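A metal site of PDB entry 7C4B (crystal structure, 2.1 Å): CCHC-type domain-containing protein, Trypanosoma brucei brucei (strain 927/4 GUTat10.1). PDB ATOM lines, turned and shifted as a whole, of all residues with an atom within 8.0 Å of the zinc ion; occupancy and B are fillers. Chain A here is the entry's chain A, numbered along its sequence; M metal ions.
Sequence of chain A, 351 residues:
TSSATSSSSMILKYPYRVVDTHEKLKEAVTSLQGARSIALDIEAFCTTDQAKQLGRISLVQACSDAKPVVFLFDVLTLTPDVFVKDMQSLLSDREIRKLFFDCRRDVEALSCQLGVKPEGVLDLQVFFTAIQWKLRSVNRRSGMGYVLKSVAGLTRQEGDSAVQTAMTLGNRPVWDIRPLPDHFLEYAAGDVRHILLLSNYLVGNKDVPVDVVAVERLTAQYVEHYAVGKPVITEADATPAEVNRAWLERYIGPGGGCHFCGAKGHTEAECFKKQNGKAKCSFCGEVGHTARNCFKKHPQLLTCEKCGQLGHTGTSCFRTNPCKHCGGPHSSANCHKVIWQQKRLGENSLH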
ATOM      1  N   LYS A 280     -14.623  -8.851  20.944  1.00  0.00           N
ATOM      2  CA  LYS A 280     -15.534  -7.936  20.254  1.00  0.00           C
ATOM      3  C   LYS A 280     -16.939  -8.215  20.756  1.00  0.00           C
ATOM      4  O   LYS A 280     -17.446  -9.330  20.630  1.00  0.00           O
ATOM      5  CB  LYS A 280     -15.452  -8.128  18.739  1.00  0.00           C
ATOM      6  CG  LYS A 280     -16.281  -7.160  17.923  1.00  0.00           C
ATOM      7  CD  LYS A 280     -16.156  -7.447  16.440  1.00  0.00           C
ATOM      8  CE  LYS A 280     -17.009  -6.509  15.611  1.00  0.00           C
ATOM      9  NZ  LYS A 280     -16.622  -5.084  15.829  1.00  0.00           N
ATOM     10  N   CYS A 281     -17.575  -7.188  21.336  1.00  0.00           N
ATOM     11  CA  CYS A 281     -18.881  -7.371  21.950  1.00  0.00           C
ATOM     12  C   CYS A 281     -19.939  -7.644  20.892  1.00  0.00           C
ATOM     13  O   CYS A 281     -20.140  -6.827  19.986  1.00  0.00           O
ATOM     14  CB  CYS A 281     -19.268  -6.151  22.782  1.00  0.00           C
ATOM     15  SG  CYS A 281     -20.888  -6.318  23.559  1.00  0.00           S
ATOM     16  N   SER A 282     -20.630  -8.776  21.008  1.00  0.00           N
ATOM     17  CA  SER A 282     -21.636  -9.149  20.031  1.00  0.00           C
ATOM     18  C   SER A 282     -22.892  -8.296  20.141  1.00  0.00           C
ATOM     19  O   SER A 282     -23.695  -8.272  19.194  1.00  0.00           O
ATOM     20  CB  SER A 282     -21.986 -10.623  20.181  1.00  0.00           C
ATOM     21  OG  SER A 282     -22.483 -10.907  21.472  1.00  0.00           O
ATOM     22  N   PHE A 283     -23.098  -7.604  21.255  1.00  0.00           N
ATOM     23  CA  PHE A 283     -24.317  -6.820  21.438  1.00  0.00           C
ATOM     24  C   PHE A 283     -24.142  -5.357  21.025  1.00  0.00           C
ATOM     25  O   PHE A 283     -25.070  -4.763  20.473  1.00  0.00           O
ATOM     26  CB  PHE A 283     -24.788  -6.890  22.897  1.00  0.00           C
ATOM     27  CG  PHE A 283     -26.085  -6.167  23.138  1.00  0.00           C
ATOM     28  CD1 PHE A 283     -27.304  -6.750  22.834  1.00  0.00           C
ATOM     29  CD2 PHE A 283     -26.086  -4.888  23.702  1.00  0.00           C
ATOM     30  CE1 PHE A 283     -28.490  -6.085  23.065  1.00  0.00           C
ATOM     31  CE2 PHE A 283     -27.271  -4.222  23.932  1.00  0.00           C
ATOM     32  CZ  PHE A 283     -28.477  -4.818  23.612  1.00  0.00           C
ATOM     33  N   CYS A 284     -22.968  -4.771  21.272  1.00  0.00           N
ATOM     34  CA  CYS A 284     -22.743  -3.361  20.974  1.00  0.00           C
ATOM     35  C   CYS A 284     -21.589  -3.117  20.009  1.00  0.00           C
ATOM     36  O   CYS A 284     -21.320  -1.960  19.658  1.00  0.00           O
ATOM     37  CB  CYS A 284     -22.490  -2.570  22.267  1.00  0.00           C
ATOM     38  SG  CYS A 284     -20.820  -2.686  22.924  1.00  0.00           S
ATOM     39  N   GLY A 285     -20.884  -4.166  19.567  1.00  0.00           N
ATOM     40  CA  GLY A 285     -19.877  -4.041  18.531  1.00  0.00           C
ATOM     41  C   GLY A 285     -18.502  -3.584  19.005  1.00  0.00           C
ATOM     42  O   GLY A 285     -17.530  -3.732  18.247  1.00  0.00           O
ATOM     43  N   GLU A 286     -18.386  -3.045  20.205  1.00  0.00           N
ATOM     44  CA  GLU A 286     -17.108  -2.521  20.675  1.00  0.00           C
ATOM     45  C   GLU A 286     -16.098  -3.648  20.857  1.00  0.00           C
ATOM     46  O   GLU A 286     -16.447  -4.766  21.234  1.00  0.00           O
ATOM     47  CB  GLU A 286     -17.299  -1.776  21.992  1.00  0.00           C
ATOM     48  CG  GLU A 286     -17.690  -0.314  21.844  1.00  0.00           C
ATOM     49  CD  GLU A 286     -18.263   0.261  23.122  1.00  0.00           C
ATOM     50  OE1 GLU A 286     -19.240   1.040  23.049  1.00  0.00           O
ATOM     51  OE2 GLU A 286     -17.739  -0.059  24.206  1.00  0.00           O
ATOM     52  N   VAL A 287     -14.839  -3.341  20.573  1.00  0.00           N
ATOM     53  CA  VAL A 287     -13.723  -4.226  20.897  1.00  0.00           C
ATOM     54  C   VAL A 287     -13.271  -3.940  22.314  1.00  0.00           C
ATOM     55  O   VAL A 287     -13.205  -2.777  22.739  1.00  0.00           O
ATOM     56  CB  VAL A 287     -12.571  -4.070  19.884  1.00  0.00           C
ATOM     57  CG1 VAL A 287     -13.017  -4.500  18.488  1.00  0.00           C
ATOM     58  CG2 VAL A 287     -12.058  -2.636  19.864  1.00  0.00           C
ATOM     59  N   GLY A 288     -12.978  -4.993  23.069  1.00  0.00           N
ATOM     60  CA  GLY A 288     -12.526  -4.817  24.436  1.00  0.00           C
ATOM     61  C   GLY A 288     -13.258  -5.657  25.458  1.00  0.00           C
ATOM     62  O   GLY A 288     -12.703  -5.972  26.512  1.00  0.00           O
ATOM     63  N   HIS A 289     -14.512  -6.017  25.176  1.00  0.00           N
ATOM     64  CA  HIS A 289     -15.294  -6.809  26.105  1.00  0.00           C
ATOM     65  C   HIS A 289     -16.232  -7.717  25.327  1.00  0.00           C
ATOM     66  O   HIS A 289     -16.454  -7.544  24.128  1.00  0.00           O
ATOM     67  CB  HIS A 289     -16.085  -5.934  27.085  1.00  0.00           C
ATOM     68  CG  HIS A 289     -17.058  -5.020  26.417  1.00  0.00           C
ATOM     69  ND1 HIS A 289     -16.710  -3.811  25.872  1.00  0.00           N
ATOM     70  CD2 HIS A 289     -18.395  -5.150  26.213  1.00  0.00           C
ATOM     71  CE1 HIS A 289     -17.777  -3.224  25.360  1.00  0.00           C
ATOM     72  NE2 HIS A 289     -18.817  -4.020  25.551  1.00  0.00           N
ATOM     73  N   THR A 290     -16.795  -8.703  26.026  1.00  0.00           N
ATOM     74  CA  THR A 290     -17.751  -9.635  25.454  1.00  0.00           C
ATOM     75  C   THR A 290     -19.160  -9.276  25.896  1.00  0.00           C
ATOM     76  O   THR A 290     -19.377  -8.418  26.749  1.00  0.00           O
ATOM     77  CB  THR A 290     -17.407 -11.070  25.871  1.00  0.00           C
ATOM     78  OG1 THR A 290     -17.368 -11.165  27.294  1.00  0.00           O
ATOM     79  CG2 THR A 290     -16.059 -11.478  25.294  1.00  0.00           C
ATOM     80  N   ALA A 291     -20.142  -9.952  25.295  1.00  0.00           N
ATOM     81  CA  ALA A 291     -21.542  -9.674  25.603  1.00  0.00           C
ATOM     82  C   ALA A 291     -21.884 -10.021  27.041  1.00  0.00           C
ATOM     83  O   ALA A 291     -22.740  -9.367  27.650  1.00  0.00           O
ATOM     84  CB  ALA A 291     -22.456 -10.433  24.651  1.00  0.00           C
ATOM     85  N   ARG A 292     -21.236 -11.036  27.612  1.00  0.00           N
ATOM     86  CA  ARG A 292     -21.473 -11.395  29.003  1.00  0.00           C
ATOM     87  C   ARG A 292     -21.055 -10.284  29.964  1.00  0.00           C
ATOM     88  O   ARG A 292     -21.552 -10.232  31.095  1.00  0.00           O
ATOM     89  CB  ARG A 292     -20.748 -12.689  29.356  1.00  0.00           C
ATOM     90  N   ASN A 293     -20.170  -9.386  29.524  1.00  0.00           N
ATOM     91  CA  ASN A 293     -19.686  -8.294  30.361  1.00  0.00           C
ATOM     92  C   ASN A 293     -20.100  -6.922  29.836  1.00  0.00           C
ATOM     93  O   ASN A 293     -19.554  -5.902  30.296  1.00  0.00           O
ATOM     94  CB  ASN A 293     -18.169  -8.371  30.496  1.00  0.00           C
ATOM     95  CG  ASN A 293     -17.693  -9.658  31.147  1.00  0.00           C
ATOM     96  OD1 ASN A 293     -18.167 -10.029  32.220  1.00  0.00           O
ATOM     97  ND2 ASN A 293     -16.777 -10.359  30.488  1.00  0.00           N
ATOM     98  N   CYS A 294     -21.040  -6.862  28.897  1.00  0.00           N
ATOM     99  CA  CYS A 294     -21.430  -5.587  28.314  1.00  0.00           C
ATOM    100  C   CYS A 294     -22.392  -4.844  29.232  1.00  0.00           C
ATOM    101  O   CYS A 294     -23.430  -5.383  29.637  1.00  0.00           O
ATOM    102  CB  CYS A 294     -22.090  -5.817  26.947  1.00  0.00           C
ATOM    103  SG  CYS A 294     -22.670  -4.298  26.146  1.00  0.00           S
ATOM    104  N   PHE A 295     -22.054  -3.597  29.567  1.00  0.00           N
ATOM    105  CA  PHE A 295     -22.940  -2.785  30.392  1.00  0.00           C
ATOM    106  C   PHE A 295     -24.212  -2.405  29.650  1.00  0.00           C
ATOM    107  O   PHE A 295     -25.272  -2.271  30.270  1.00  0.00           O
ATOM    108  CB  PHE A 295     -22.211  -1.523  30.867  1.00  0.00           C
ATOM    109  CG  PHE A 295     -20.908  -1.802  31.561  1.00  0.00           C
ATOM    110  CD1 PHE A 295     -20.871  -2.481  32.770  1.00  0.00           C
ATOM    111  CD2 PHE A 295     -19.712  -1.370  30.998  1.00  0.00           C
ATOM    112  CE1 PHE A 295     -19.669  -2.732  33.399  1.00  0.00           C
ATOM    113  CE2 PHE A 295     -18.502  -1.625  31.632  1.00  0.00           C
ATOM    114  CZ  PHE A 295     -18.485  -2.304  32.830  1.00  0.00           C
ATOM    115  N   LYS A 296     -24.131  -2.232  28.328  1.00  0.00           N
ATOM    116  CA  LYS A 296     -25.314  -1.883  27.553  1.00  0.00           C
ATOM    117  C   LYS A 296     -26.320  -3.021  27.536  1.00  0.00           C
ATOM    118  O   LYS A 296     -27.535  -2.786  27.658  1.00  0.00           O
ATOM    119  CB  LYS A 296     -24.915  -1.496  26.124  1.00  0.00           C
ATOM    120  N   LYS A 297     -25.844  -4.264  27.396  1.00  0.00           N
ATOM    121  CA  LYS A 297     -26.752  -5.402  27.386  1.00  0.00           C
ATOM    122  C   LYS A 297     -27.207  -5.771  28.797  1.00  0.00           C
ATOM    123  O   LYS A 297     -28.361  -6.178  28.986  1.00  0.00           O
ATOM    124  CB  LYS A 297     -26.073  -6.605  26.721  1.00  0.00           C
ATOM    125  CG  LYS A 297     -26.960  -7.833  26.593  1.00  0.00           C
ATOM    126  CD  LYS A 297     -26.312  -8.886  25.713  1.00  0.00           C
ATOM    127  CE  LYS A 297     -27.196 -10.119  25.599  1.00  0.00           C
ATOM    128  NZ  LYS A 297     -26.634 -11.117  24.652  1.00  0.00           N
ATOM    129  N   HIS A 298     -26.329  -5.627  29.789  1.00  0.00           N
ATOM    130  CA  HIS A 298     -26.623  -5.981  31.173  1.00  0.00           C
ATOM    131  C   HIS A 298     -26.440  -4.742  32.048  1.00  0.00           C
ATOM    132  O   HIS A 298     -25.368  -4.545  32.646  1.00  0.00           O
ATOM    133  CB  HIS A 298     -25.722  -7.126  31.647  1.00  0.00           C
ATOM    134  CG  HIS A 298     -25.756  -8.323  30.751  1.00  0.00           C
ATOM    135  ND1 HIS A 298     -26.781  -9.253  30.787  1.00  0.00           N
ATOM    136  CD2 HIS A 298     -24.894  -8.743  29.801  1.00  0.00           C
ATOM    137  CE1 HIS A 298     -26.541 -10.190  29.897  1.00  0.00           C
ATOM    138  NE2 HIS A 298     -25.403  -9.908  29.277  1.00  0.00           N
HETATM  139 ZN    ZN M   1     -20.992  -4.288  24.557  1.00  0.00          ZN
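The side-chain sulfur (SG) of Cys 281 lies close to the backbone NH (N) of Phe 283 (3.4 Å).
The backbone carbonyl oxygen (O) of Glu 286 is in hydrogen-bond range of the backbone NH (N) of Cys 281.
The side-chain sulfur of Cys 284 lies close to the backbone NH of Glu 286, at 3.7 Å.
SG of Cys 294 sits close to N of Lys 296 (3.3 Å).
The side-chain sulfur (SG) of Cys 294 lies close to the backbone NH (N) of Lys 297, 3.4 Å away.
The nearest printed residue that does not touch the zinc ion is Phe 283 (4.9 Å).
The zinc ion is bound by the side-chain sulfur (SG) of Cys 281, the side-chain sulfur (SG) of Cys 284, the side-chain sulfur (SG) of Cys 294 and a ring nitrogen (NE2) of His 289.
The zinc ion has four donor atoms within binding distance.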
